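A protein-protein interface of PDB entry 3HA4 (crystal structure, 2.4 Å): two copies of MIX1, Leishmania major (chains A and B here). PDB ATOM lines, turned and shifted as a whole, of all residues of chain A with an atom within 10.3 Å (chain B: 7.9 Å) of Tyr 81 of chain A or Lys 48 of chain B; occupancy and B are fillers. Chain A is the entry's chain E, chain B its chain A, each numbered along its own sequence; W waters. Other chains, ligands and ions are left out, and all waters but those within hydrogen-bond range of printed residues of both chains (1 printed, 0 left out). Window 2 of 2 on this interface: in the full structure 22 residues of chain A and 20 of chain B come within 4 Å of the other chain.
Arg 45 of chain B touches its own counterpart, Arg 45 of chain A. Arg 45 of chain A touches Glu 46 of chain B, and with the chains exchanged Glu 46 of chain A touches Arg 45 of chain B. 4 positions are printed for both chains.
Among the printed residues, merely in contact across the chains: Tyr 81 of chain A with Glu 46 of chain B, Tyr 81 of chain A with Leu 43 of chain B, Arg 45 of chain A with Arg 45 of chain B and Tyr 81 of chain A with Lys 48 of chain B.
The backbone NH of Lys 48 of chain B sits at hydrogen-bond distance from the backbone carbonyl oxygen of Leu 43 of chain B (3.1 Å). The backbone carbonyl oxygen (O) of Leu 43 of chain B sits at hydrogen-bond distance from the backbone NH (N) of Gly 49 of chain B (3.4 Å). NH1 of Arg 45 of chain A is in salt-bridge range of OE2 of Glu 74 of chain A (3.3 Å).
Water W1 lies within hydrogen-bond range of OE1 of Glu 74 of chain A (2.9 Å), NH1 of Arg 45 of chain A (3.4 Å) and NH1 of Arg 45 of chain B (3.5 Å).
Hydrophobic or aromatic side chains of chain B that line the printed part of chain A: Leu 43. Hydrophobic or aromatic side chains of chain A that line the printed part of chain B: Tyr 81 and Met 131.
NH2 of Arg 45 of chain B is in salt-bridge range of OE2 of Glu 74 of chain A (2.4 Å). The side-chain carboxylate (OE1) of Glu 46 of chain B is in salt-bridge range of the guanidinium group (NH2) of Arg 45 of chain A. The side-chain carboxylate of Glu 46 of chain A is in salt-bridge range of the guanidinium group of Arg 45 of chain B, 3.3 Å away. The side-chain amide oxygen (OE1) of Gln 39 of chain B lies close to the side-chain sulfur (SD) of Met 131 of chain A, 3.7 Å away.
Of the printed residues of chain B, Arg 45 of chain A touches Arg 45 (3.8 Å) and Glu 46 (3.0 Å). Val 78 of chain A touches none of the printed residues of chain B. No residue of chain B comes within 4 Å of Lys 80 of chain A. Tyr 81 of chain A touches just these residues of chain B: Leu 43 (3.7 Å), Glu 46 (3.5 Å) and Lys 48 (3.8 Å). Met 139 of chain A touches none of the printed residues of chain B. Printed residues of chain A within 4 Å of Arg 45 of chain B: Arg 45, Glu 46 and Glu 74. Of chain A, only Arg 45 (3.0 Å) and Tyr 81 (3.5 Å) come within 4 Å of Glu 46 of chain B. Of chain A, only Tyr 81 (3.8 Å) comes within 4 Å of Lys 48 of chain B. No residue of chain A comes within 4 Å of Gly 49 of chain B. The nearest residue of chain A that does not touch Lys 48 of chain B is Lys 80 of chain A (6.8 Å).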
ATOM      1  N   LEU A  44      33.281 -24.097  20.959  1.00  0.00           N
ATOM      2  CA  LEU A  44      32.335 -23.633  21.941  1.00  0.00           C
ATOM      3  C   LEU A  44      31.355 -22.677  21.319  1.00  0.00           C
ATOM      4  O   LEU A  44      30.202 -22.642  21.681  1.00  0.00           O
ATOM      5  CB  LEU A  44      33.071 -23.014  23.131  1.00  0.00           C
ATOM      6  CG  LEU A  44      32.380 -22.099  24.120  1.00  0.00           C
ATOM      7  CD1 LEU A  44      33.019 -20.753  23.978  1.00  0.00           C
ATOM      8  CD2 LEU A  44      30.949 -22.014  23.761  1.00  0.00           C
ATOM      9  N   ARG A  45      31.819 -21.913  20.355  1.00  0.00           N
ATOM     10  CA  ARG A  45      30.931 -21.044  19.625  1.00  0.00           C
ATOM     11  C   ARG A  45      30.053 -21.844  18.675  1.00  0.00           C
ATOM     12  O   ARG A  45      28.935 -21.492  18.409  1.00  0.00           O
ATOM     13  CB  ARG A  45      31.740 -20.019  18.861  1.00  0.00           C
ATOM     14  CG  ARG A  45      31.059 -19.526  17.655  1.00  0.00           C
ATOM     15  CD  ARG A  45      31.481 -18.158  17.295  1.00  0.00           C
ATOM     16  NE  ARG A  45      30.473 -17.561  16.451  1.00  0.00           N
ATOM     17  CZ  ARG A  45      30.678 -17.065  15.245  1.00  0.00           C
ATOM     18  NH1 ARG A  45      31.860 -17.068  14.706  1.00  0.00           N
ATOM     19  NH2 ARG A  45      29.678 -16.553  14.591  1.00  0.00           N
ATOM     20  N   GLU A  46      30.571 -22.946  18.181  1.00  0.00           N
ATOM     21  CA  GLU A  46      29.824 -23.761  17.268  1.00  0.00           C
ATOM     22  C   GLU A  46      28.943 -24.727  18.002  1.00  0.00           C
ATOM     23  O   GLU A  46      28.372 -25.602  17.390  1.00  0.00           O
ATOM     24  CB  GLU A  46      30.745 -24.520  16.329  1.00  0.00           C
ATOM     25  CG  GLU A  46      31.286 -23.706  15.190  1.00  0.00           C
ATOM     26  CD  GLU A  46      30.222 -23.066  14.376  1.00  0.00           C
ATOM     27  OE1 GLU A  46      30.267 -21.861  14.163  1.00  0.00           O
ATOM     28  OE2 GLU A  46      29.335 -23.773  13.940  1.00  0.00           O
ATOM     29  N   LEU A  73      39.365 -12.168  18.859  1.00  0.00           N
ATOM     30  CA  LEU A  73      38.411 -11.984  17.755  1.00  0.00           C
ATOM     31  C   LEU A  73      37.318 -13.052  17.741  1.00  0.00           C
ATOM     32  O   LEU A  73      36.144 -12.731  17.547  1.00  0.00           O
ATOM     33  CB  LEU A  73      39.102 -11.905  16.379  1.00  0.00           C
ATOM     34  CG  LEU A  73      39.405 -10.497  15.847  1.00  0.00           C
ATOM     35  CD1 LEU A  73      40.199  -9.687  16.863  1.00  0.00           C
ATOM     36  CD2 LEU A  73      40.130 -10.535  14.495  1.00  0.00           C
ATOM     37  N   GLU A  74      37.683 -14.315  17.944  1.00  0.00           N
ATOM     38  CA  GLU A  74      36.660 -15.350  17.922  1.00  0.00           C
ATOM     39  C   GLU A  74      35.698 -15.155  19.074  1.00  0.00           C
ATOM     40  O   GLU A  74      34.487 -15.371  18.933  1.00  0.00           O
ATOM     41  CB  GLU A  74      37.250 -16.747  18.003  1.00  0.00           C
ATOM     42  CG  GLU A  74      36.177 -17.814  17.796  1.00  0.00           C
ATOM     43  CD  GLU A  74      35.677 -17.855  16.363  1.00  0.00           C
ATOM     44  OE1 GLU A  74      36.432 -17.415  15.471  1.00  0.00           O
ATOM     45  OE2 GLU A  74      34.539 -18.322  16.126  1.00  0.00           O
ATOM     46  N   LEU A  75      36.259 -14.748  20.211  1.00  0.00           N
ATOM     47  CA  LEU A  75      35.515 -14.543  21.444  1.00  0.00           C
ATOM     48  C   LEU A  75      34.514 -13.412  21.268  1.00  0.00           C
ATOM     49  O   LEU A  75      33.377 -13.480  21.752  1.00  0.00           O
ATOM     50  CB  LEU A  75      36.481 -14.214  22.575  1.00  0.00           C
ATOM     51  CG  LEU A  75      36.371 -15.121  23.797  1.00  0.00           C
ATOM     52  CD1 LEU A  75      36.347 -16.579  23.371  1.00  0.00           C
ATOM     53  CD2 LEU A  75      37.529 -14.860  24.738  1.00  0.00           C
ATOM     54  N   THR A  76      34.942 -12.372  20.561  1.00  0.00           N
ATOM     55  CA  THR A  76      34.075 -11.236  20.286  1.00  0.00           C
ATOM     56  C   THR A  76      32.838 -11.683  19.527  1.00  0.00           C
ATOM     57  O   THR A  76      31.739 -11.177  19.758  1.00  0.00           O
ATOM     58  CB  THR A  76      34.815 -10.155  19.480  1.00  0.00           C
ATOM     59  OG1 THR A  76      35.937  -9.688  20.246  1.00  0.00           O
ATOM     60  CG2 THR A  76      33.880  -8.982  19.149  1.00  0.00           C
ATOM     61  N   GLN A  77      33.017 -12.642  18.623  1.00  0.00           N
ATOM     62  CA  GLN A  77      31.882 -13.190  17.887  1.00  0.00           C
ATOM     63  C   GLN A  77      30.933 -13.942  18.821  1.00  0.00           C
ATOM     64  O   GLN A  77      29.712 -13.851  18.682  1.00  0.00           O
ATOM     65  CB  GLN A  77      32.362 -14.099  16.748  1.00  0.00           C
ATOM     66  CG  GLN A  77      33.351 -13.429  15.806  1.00  0.00           C
ATOM     67  CD  GLN A  77      32.817 -12.140  15.221  1.00  0.00           C
ATOM     68  OE1 GLN A  77      31.721 -12.109  14.656  1.00  0.00           O
ATOM     69  NE2 GLN A  77      33.586 -11.064  15.359  1.00  0.00           N
ATOM     70  N   VAL A  78      31.497 -14.685  19.769  1.00  0.00           N
ATOM     71  CA  VAL A  78      30.671 -15.378  20.743  1.00  0.00           C
ATOM     72  C   VAL A  78      29.818 -14.351  21.470  1.00  0.00           C
ATOM     73  O   VAL A  78      28.593 -14.461  21.513  1.00  0.00           O
ATOM     74  CB  VAL A  78      31.507 -16.128  21.782  1.00  0.00           C
ATOM     75  CG1 VAL A  78      30.590 -16.793  22.794  1.00  0.00           C
ATOM     76  CG2 VAL A  78      32.410 -17.152  21.114  1.00  0.00           C
ATOM     77  N   LEU A  79      30.485 -13.349  22.029  1.00  0.00           N
ATOM     78  CA  LEU A  79      29.816 -12.278  22.742  1.00  0.00           C
ATOM     79  C   LEU A  79      28.787 -11.632  21.832  1.00  0.00           C
ATOM     80  O   LEU A  79      27.617 -11.509  22.183  1.00  0.00           O
ATOM     81  CB  LEU A  79      30.834 -11.230  23.199  1.00  0.00           C
ATOM     82  CG  LEU A  79      31.956 -11.753  24.103  1.00  0.00           C
ATOM     83  CD1 LEU A  79      32.934 -10.650  24.473  1.00  0.00           C
ATOM     84  CD2 LEU A  79      31.373 -12.390  25.359  1.00  0.00           C
ATOM     85  N   LYS A  80      29.238 -11.235  20.648  1.00  0.00           N
ATOM     86  CA  LYS A  80      28.414 -10.495  19.709  1.00  0.00           C
ATOM     87  C   LYS A  80      27.097 -11.201  19.411  1.00  0.00           C
ATOM     88  O   LYS A  80      26.054 -10.554  19.308  1.00  0.00           O
ATOM     89  CB  LYS A  80      29.194 -10.256  18.412  1.00  0.00           C
ATOM     90  CG  LYS A  80      28.448  -9.452  17.363  1.00  0.00           C
ATOM     91  CD  LYS A  80      29.319  -9.220  16.137  1.00  0.00           C
ATOM     92  CE  LYS A  80      28.741  -8.124  15.249  1.00  0.00           C
ATOM     93  NZ  LYS A  80      29.649  -7.790  14.119  1.00  0.00           N
ATOM     94  N   TYR A  81      27.122 -12.502  19.260  1.00  0.00           N
ATOM     95  CA  TYR A  81      25.947 -13.178  18.785  1.00  0.00           C
ATOM     96  C   TYR A  81      25.305 -14.142  19.749  1.00  0.00           C
ATOM     97  O   TYR A  81      24.421 -14.884  19.372  1.00  0.00           O
ATOM     98  CB  TYR A  81      26.286 -13.929  17.531  1.00  0.00           C
ATOM     99  CG  TYR A  81      26.722 -13.078  16.396  1.00  0.00           C
ATOM    100  CD1 TYR A  81      25.862 -12.203  15.806  1.00  0.00           C
ATOM    101  CD2 TYR A  81      27.990 -13.186  15.889  1.00  0.00           C
ATOM    102  CE1 TYR A  81      26.257 -11.447  14.760  1.00  0.00           C
ATOM    103  CE2 TYR A  81      28.385 -12.441  14.857  1.00  0.00           C
ATOM    104  CZ  TYR A  81      27.523 -11.572  14.292  1.00  0.00           C
ATOM    105  OH  TYR A  81      27.920 -10.821  13.245  1.00  0.00           O
ATOM    106  N   SER A  82      25.761 -14.147  20.987  1.00  0.00           N
ATOM    107  CA  SER A  82      25.156 -14.977  22.001  1.00  0.00           C
ATOM    108  C   SER A  82      24.041 -14.207  22.654  1.00  0.00           C
ATOM    109  O   SER A  82      24.015 -13.006  22.634  1.00  0.00           O
ATOM    110  CB  SER A  82      26.185 -15.420  23.023  1.00  0.00           C
ATOM    111  OG  SER A  82      26.877 -16.537  22.543  1.00  0.00           O
ATOM    112  N   SER A  83      23.100 -14.923  23.221  1.00  0.00           N
ATOM    113  CA  SER A  83      21.946 -14.292  23.790  1.00  0.00           C
ATOM    114  C   SER A  83      22.215 -13.962  25.226  1.00  0.00           C
ATOM    115  O   SER A  83      22.940 -14.669  25.886  1.00  0.00           O
ATOM    116  CB  SER A  83      20.763 -15.231  23.695  1.00  0.00           C
ATOM    117  OG  SER A  83      21.078 -16.481  24.254  1.00  0.00           O
ATOM    118  N   GLY A  84      21.620 -12.887  25.714  1.00  0.00           N
ATOM    119  CA  GLY A  84      21.741 -12.553  27.114  1.00  0.00           C
ATOM    120  C   GLY A  84      21.433 -13.765  27.961  1.00  0.00           C
ATOM    121  O   GLY A  84      22.101 -14.046  28.929  1.00  0.00           O
ATOM    122  N   LYS A  85      20.405 -14.486  27.567  1.00  0.00           N
ATOM    123  CA  LYS A  85      20.108 -15.763  28.136  1.00  0.00           C
ATOM    124  C   LYS A  85      21.367 -16.587  28.282  1.00  0.00           C
ATOM    125  O   LYS A  85      21.823 -16.826  29.368  1.00  0.00           O
ATOM    126  CB  LYS A  85      19.139 -16.491  27.220  1.00  0.00           C
ATOM    127  CG  LYS A  85      17.911 -17.055  27.900  1.00  0.00           C
ATOM    128  CD  LYS A  85      16.622 -16.465  27.331  1.00  0.00           C
ATOM    129  CE  LYS A  85      15.845 -15.706  28.403  1.00  0.00           C
ATOM    130  NZ  LYS A  85      15.117 -14.536  27.877  1.00  0.00           N
ATOM    131  N   TYR A  86      21.916 -17.026  27.161  1.00  0.00           N
ATOM    132  CA  TYR A  86      23.052 -17.926  27.125  1.00  0.00           C
ATOM    133  C   TYR A  86      24.202 -17.370  27.872  1.00  0.00           C
ATOM    134  O   TYR A  86      24.936 -18.057  28.536  1.00  0.00           O
ATOM    135  CB  TYR A  86      23.482 -18.083  25.683  1.00  0.00           C
ATOM    136  CG  TYR A  86      24.794 -18.782  25.455  1.00  0.00           C
ATOM    137  CD1 TYR A  86      24.831 -20.045  24.911  1.00  0.00           C
ATOM    138  CD2 TYR A  86      25.983 -18.173  25.733  1.00  0.00           C
ATOM    139  CE1 TYR A  86      25.996 -20.665  24.679  1.00  0.00           C
ATOM    140  CE2 TYR A  86      27.151 -18.802  25.497  1.00  0.00           C
ATOM    141  CZ  TYR A  86      27.143 -20.039  24.969  1.00  0.00           C
ATOM    142  OH  TYR A  86      28.291 -20.685  24.744  1.00  0.00           O
ATOM    143  N   LEU A  87      24.369 -16.091  27.704  1.00  0.00           N
ATOM    144  CA  LEU A  87      25.537 -15.401  28.220  1.00  0.00           C
ATOM    145  C   LEU A  87      25.560 -15.455  29.741  1.00  0.00           C
ATOM    146  O   LEU A  87      26.582 -15.764  30.347  1.00  0.00           O
ATOM    147  CB  LEU A  87      25.552 -13.956  27.718  1.00  0.00           C
ATOM    148  CG  LEU A  87      26.862 -13.444  27.117  1.00  0.00           C
ATOM    149  CD1 LEU A  87      27.619 -14.568  26.427  1.00  0.00           C
ATOM    150  CD2 LEU A  87      26.572 -12.316  26.144  1.00  0.00           C
ATOM    151  N   MET A 131      38.071  -3.471  13.920  1.00  0.00           N
ATOM    152  CA  MET A 131      36.700  -3.883  13.644  1.00  0.00           C
ATOM    153  C   MET A 131      36.126  -4.617  14.845  1.00  0.00           C
ATOM    154  O   MET A 131      34.939  -4.482  15.168  1.00  0.00           O
ATOM    155  CB  MET A 131      36.657  -4.809  12.430  1.00  0.00           C
ATOM    156  CG  MET A 131      36.770  -4.111  11.090  1.00  0.00           C
ATOM    157  SD  MET A 131      37.064  -5.288   9.757  1.00  0.00           S
ATOM    158  CE  MET A 131      36.449  -4.337   8.357  1.00  0.00           C
ATOM    159  N   ASP A 135      33.028  -3.703  17.357  1.00  0.00           N
ATOM    160  CA  ASP A 135      31.958  -4.594  17.792  1.00  0.00           C
ATOM    161  C   ASP A 135      31.882  -4.617  19.326  1.00  0.00           C
ATOM    162  O   ASP A 135      30.801  -4.581  19.903  1.00  0.00           O
ATOM    163  CB  ASP A 135      32.154  -6.019  17.231  1.00  0.00           C
ATOM    164  CG  ASP A 135      32.046  -6.086  15.699  1.00  0.00           C
ATOM    165  OD1 ASP A 135      31.736  -5.053  15.065  1.00  0.00           O
ATOM    166  OD2 ASP A 135      32.277  -7.178  15.124  1.00  0.00           O
ATOM    167  N   LEU A 136      33.038  -4.664  19.983  1.00  0.00           N
ATOM    168  CA  LEU A 136      33.089  -4.740  21.440  1.00  0.00           C
ATOM    169  C   LEU A 136      32.510  -3.509  22.130  1.00  0.00           C
ATOM    170  O   LEU A 136      31.888  -3.614  23.187  1.00  0.00           O
ATOM    171  CB  LEU A 136      34.517  -4.977  21.915  1.00  0.00           C
ATOM    172  CG  LEU A 136      35.048  -6.385  21.667  1.00  0.00           C
ATOM    173  CD1 LEU A 136      36.512  -6.481  22.090  1.00  0.00           C
ATOM    174  CD2 LEU A 136      34.184  -7.414  22.397  1.00  0.00           C
ATOM    175  N   ASN A 138      30.221  -1.395  20.784  1.00  0.00           N
ATOM    176  CA  ASN A 138      28.802  -1.267  20.473  1.00  0.00           C
ATOM    177  C   ASN A 138      27.975  -2.385  21.091  1.00  0.00           C
ATOM    178  O   ASN A 138      26.919  -2.750  20.575  1.00  0.00           O
ATOM    179  CB  ASN A 138      28.584  -1.263  18.956  1.00  0.00           C
ATOM    180  CG  ASN A 138      28.583   0.139  18.361  1.00  0.00           C
ATOM    181  OD1 ASN A 138      29.373   0.447  17.464  1.00  0.00           O
ATOM    182  ND2 ASN A 138      27.684   0.993  18.850  1.00  0.00           N
ATOM    183  N   MET A 139      28.452  -2.931  22.202  1.00  0.00           N
ATOM    184  CA  MET A 139      27.823  -4.115  22.761  1.00  0.00           C
ATOM    185  C   MET A 139      27.208  -3.846  24.134  1.00  0.00           C
ATOM    186  O   MET A 139      27.916  -3.530  25.089  1.00  0.00           O
ATOM    187  CB  MET A 139      28.845  -5.247  22.839  1.00  0.00           C
ATOM    188  CG  MET A 139      28.341  -6.570  22.290  1.00  0.00           C
ATOM    189  SD  MET A 139      29.577  -7.874  22.420  1.00  0.00           S
ATOM    190  CE  MET A 139      30.856  -7.241  21.343  1.00  0.00           C
ATOM    191  N   GLN B  39      36.108  -9.659   7.105  1.00  0.00           N
ATOM    192  CA  GLN B  39      34.868  -9.347   7.803  1.00  0.00           C
ATOM    193  C   GLN B  39      33.627  -9.978   7.143  1.00  0.00           C
ATOM    194  O   GLN B  39      32.710 -10.437   7.830  1.00  0.00           O
ATOM    195  CB  GLN B  39      34.711  -7.837   7.953  1.00  0.00           C
ATOM    196  CG  GLN B  39      33.484  -7.397   8.723  1.00  0.00           C
ATOM    197  CD  GLN B  39      33.355  -5.881   8.767  1.00  0.00           C
ATOM    198  OE1 GLN B  39      33.323  -5.274   9.837  1.00  0.00           O
ATOM    199  NE2 GLN B  39      33.305  -5.262   7.595  1.00  0.00           N
ATOM    200  N   ARG B  40      33.621 -10.065   5.835  1.00  0.00           N
ATOM    201  CA  ARG B  40      32.524 -10.651   5.124  1.00  0.00           C
ATOM    202  C   ARG B  40      32.485 -12.141   5.272  1.00  0.00           C
ATOM    203  O   ARG B  40      31.458 -12.748   5.328  1.00  0.00           O
ATOM    204  CB  ARG B  40      32.646 -10.288   3.674  1.00  0.00           C
ATOM    205  CG  ARG B  40      31.806  -9.175   3.308  1.00  0.00           C
ATOM    206  CD  ARG B  40      32.154  -8.515   2.048  1.00  0.00           C
ATOM    207  NE  ARG B  40      31.567  -7.198   2.067  1.00  0.00           N
ATOM    208  CZ  ARG B  40      31.445  -6.398   1.023  1.00  0.00           C
ATOM    209  NH1 ARG B  40      31.879  -6.771  -0.152  1.00  0.00           N
ATOM    210  NH2 ARG B  40      30.889  -5.226   1.157  1.00  0.00           N
ATOM    211  N   VAL B  42      33.688 -13.772   7.809  1.00  0.00           N
ATOM    212  CA  VAL B  42      33.435 -14.096   9.180  1.00  0.00           C
ATOM    213  C   VAL B  42      31.974 -14.064   9.571  1.00  0.00           C
ATOM    214  O   VAL B  42      31.607 -14.640  10.547  1.00  0.00           O
ATOM    215  CB  VAL B  42      34.231 -13.219  10.101  1.00  0.00           C
ATOM    216  CG1 VAL B  42      33.758 -13.359  11.440  1.00  0.00           C
ATOM    217  CG2 VAL B  42      35.628 -13.564  10.046  1.00  0.00           C
ATOM    218  N   LEU B  43      31.176 -13.392   8.785  1.00  0.00           N
ATOM    219  CA  LEU B  43      29.763 -13.284   8.969  1.00  0.00           C
ATOM    220  C   LEU B  43      29.107 -14.579   8.600  1.00  0.00           C
ATOM    221  O   LEU B  43      28.038 -14.867   9.024  1.00  0.00           O
ATOM    222  CB  LEU B  43      29.259 -12.229   8.024  1.00  0.00           C
ATOM    223  CG  LEU B  43      28.503 -10.956   8.309  1.00  0.00           C
ATOM    224  CD1 LEU B  43      28.608 -10.417   9.657  1.00  0.00           C
ATOM    225  CD2 LEU B  43      28.948 -10.000   7.327  1.00  0.00           C
ATOM    226  N   LEU B  44      29.766 -15.366   7.789  1.00  0.00           N
ATOM    227  CA  LEU B  44      29.152 -16.541   7.250  1.00  0.00           C
ATOM    228  C   LEU B  44      28.841 -17.604   8.262  1.00  0.00           C
ATOM    229  O   LEU B  44      27.815 -18.201   8.197  1.00  0.00           O
ATOM    230  CB  LEU B  44      30.001 -17.135   6.147  1.00  0.00           C
ATOM    231  CG  LEU B  44      30.061 -16.423   4.829  1.00  0.00           C
ATOM    232  CD1 LEU B  44      31.168 -16.978   4.054  1.00  0.00           C
ATOM    233  CD2 LEU B  44      28.836 -16.658   4.157  1.00  0.00           C
ATOM    234  N   ARG B  45      29.735 -17.858   9.186  1.00  0.00           N
ATOM    235  CA  ARG B  45      29.528 -18.925  10.130  1.00  0.00           C
ATOM    236  C   ARG B  45      28.404 -18.660  11.084  1.00  0.00           C
ATOM    237  O   ARG B  45      27.944 -19.543  11.757  1.00  0.00           O
ATOM    238  CB  ARG B  45      30.790 -19.193  10.911  1.00  0.00           C
ATOM    239  CG  ARG B  45      31.142 -20.644  11.012  1.00  0.00           C
ATOM    240  CD  ARG B  45      32.595 -20.785  11.223  1.00  0.00           C
ATOM    241  NE  ARG B  45      32.974 -20.697  12.619  1.00  0.00           N
ATOM    242  CZ  ARG B  45      33.976 -19.970  13.078  1.00  0.00           C
ATOM    243  NH1 ARG B  45      34.720 -19.242  12.275  1.00  0.00           N
ATOM    244  NH2 ARG B  45      34.217 -19.970  14.357  1.00  0.00           N
ATOM    245  N   GLU B  46      27.961 -17.428  11.148  1.00  0.00           N
ATOM    246  CA  GLU B  46      26.874 -17.080  12.019  1.00  0.00           C
ATOM    247  C   GLU B  46      25.592 -16.933  11.252  1.00  0.00           C
ATOM    248  O   GLU B  46      24.595 -16.518  11.794  1.00  0.00           O
ATOM    249  CB  GLU B  46      27.174 -15.786  12.736  1.00  0.00           C
ATOM    250  CG  GLU B  46      26.032 -15.294  13.524  1.00  0.00           C
ATOM    251  CD  GLU B  46      25.827 -16.070  14.780  1.00  0.00           C
ATOM    252  OE1 GLU B  46      26.804 -16.549  15.319  1.00  0.00           O
ATOM    253  OE2 GLU B  46      24.696 -16.203  15.229  1.00  0.00           O
ATOM    254  N   GLY B  47      25.633 -17.278   9.979  1.00  0.00           N
ATOM    255  CA  GLY B  47      24.498 -17.173   9.102  1.00  0.00           C
ATOM    256  C   GLY B  47      24.018 -15.761   8.936  1.00  0.00           C
ATOM    257  O   GLY B  47      22.843 -15.525   8.900  1.00  0.00           O
ATOM    258  N   LYS B  48      24.920 -14.816   8.826  1.00  0.00           N
ATOM    259  CA  LYS B  48      24.537 -13.432   8.718  1.00  0.00           C
ATOM    260  C   LYS B  48      25.183 -12.773   7.519  1.00  0.00           C
ATOM    261  O   LYS B  48      25.082 -11.568   7.329  1.00  0.00           O
ATOM    262  CB  LYS B  48      24.951 -12.693   9.968  1.00  0.00           C
ATOM    263  CG  LYS B  48      23.909 -12.658  11.025  1.00  0.00           C
ATOM    264  CD  LYS B  48      23.929 -11.349  11.740  1.00  0.00           C
ATOM    265  CE  LYS B  48      22.852 -11.305  12.782  1.00  0.00           C
ATOM    266  NZ  LYS B  48      22.096 -12.564  12.822  1.00  0.00           N
ATOM    267  N   GLY B  49      25.835 -13.582   6.706  1.00  0.00           N
ATOM    268  CA  GLY B  49      26.592 -13.068   5.609  1.00  0.00           C
ATOM    269  C   GLY B  49      25.922 -13.250   4.302  1.00  0.00           C
ATOM    270  O   GLY B  49      24.750 -13.367   4.229  1.00  0.00           O
ATOM    271  N   ALA B  50      26.712 -13.239   3.256  1.00  0.00           N
ATOM    272  CA  ALA B  50      26.240 -13.507   1.933  1.00  0.00           C
ATOM    273  C   ALA B  50      26.831 -14.795   1.422  1.00  0.00           C
ATOM    274  O   ALA B  50      27.813 -14.800   0.777  1.00  0.00           O
ATOM    275  CB  ALA B  50      26.567 -12.417   1.067  1.00  0.00           C
ATOM    276  N   PRO B  51      26.187 -15.895   1.735  1.00  0.00           N
ATOM    277  CA  PRO B  51      26.652 -17.206   1.363  1.00  0.00           C
ATOM    278  C   PRO B  51      26.569 -17.465  -0.113  1.00  0.00           C
ATOM    279  O   PRO B  51      27.276 -18.256  -0.646  1.00  0.00           O
ATOM    280  CB  PRO B  51      25.689 -18.086   2.108  1.00  0.00           C
ATOM    281  CG  PRO B  51      24.611 -17.272   2.408  1.00  0.00           C
ATOM    282  CD  PRO B  51      25.149 -16.028   2.742  1.00  0.00           C
ATOM    283  N   TYR B  86      23.502 -27.030   2.915  1.00  0.00           N
ATOM    284  CA  TYR B  86      23.840 -25.618   2.916  1.00  0.00           C
ATOM    285  C   TYR B  86      24.970 -25.361   1.935  1.00  0.00           C
ATOM    286  O   TYR B  86      24.846 -24.502   1.062  1.00  0.00           O
ATOM    287  CB  TYR B  86      24.228 -25.187   4.328  1.00  0.00           C
ATOM    288  CG  TYR B  86      24.764 -23.781   4.459  1.00  0.00           C
ATOM    289  CD1 TYR B  86      23.949 -22.746   4.924  1.00  0.00           C
ATOM    290  CD2 TYR B  86      26.090 -23.490   4.160  1.00  0.00           C
ATOM    291  CE1 TYR B  86      24.437 -21.451   5.071  1.00  0.00           C
ATOM    292  CE2 TYR B  86      26.587 -22.202   4.297  1.00  0.00           C
ATOM    293  CZ  TYR B  86      25.760 -21.187   4.752  1.00  0.00           C
ATOM    294  OH  TYR B  86      26.268 -19.912   4.892  1.00  0.00           O
HETATM  295  O   HOH W   1      34.811 -15.994  13.477  1.00  0.00           O
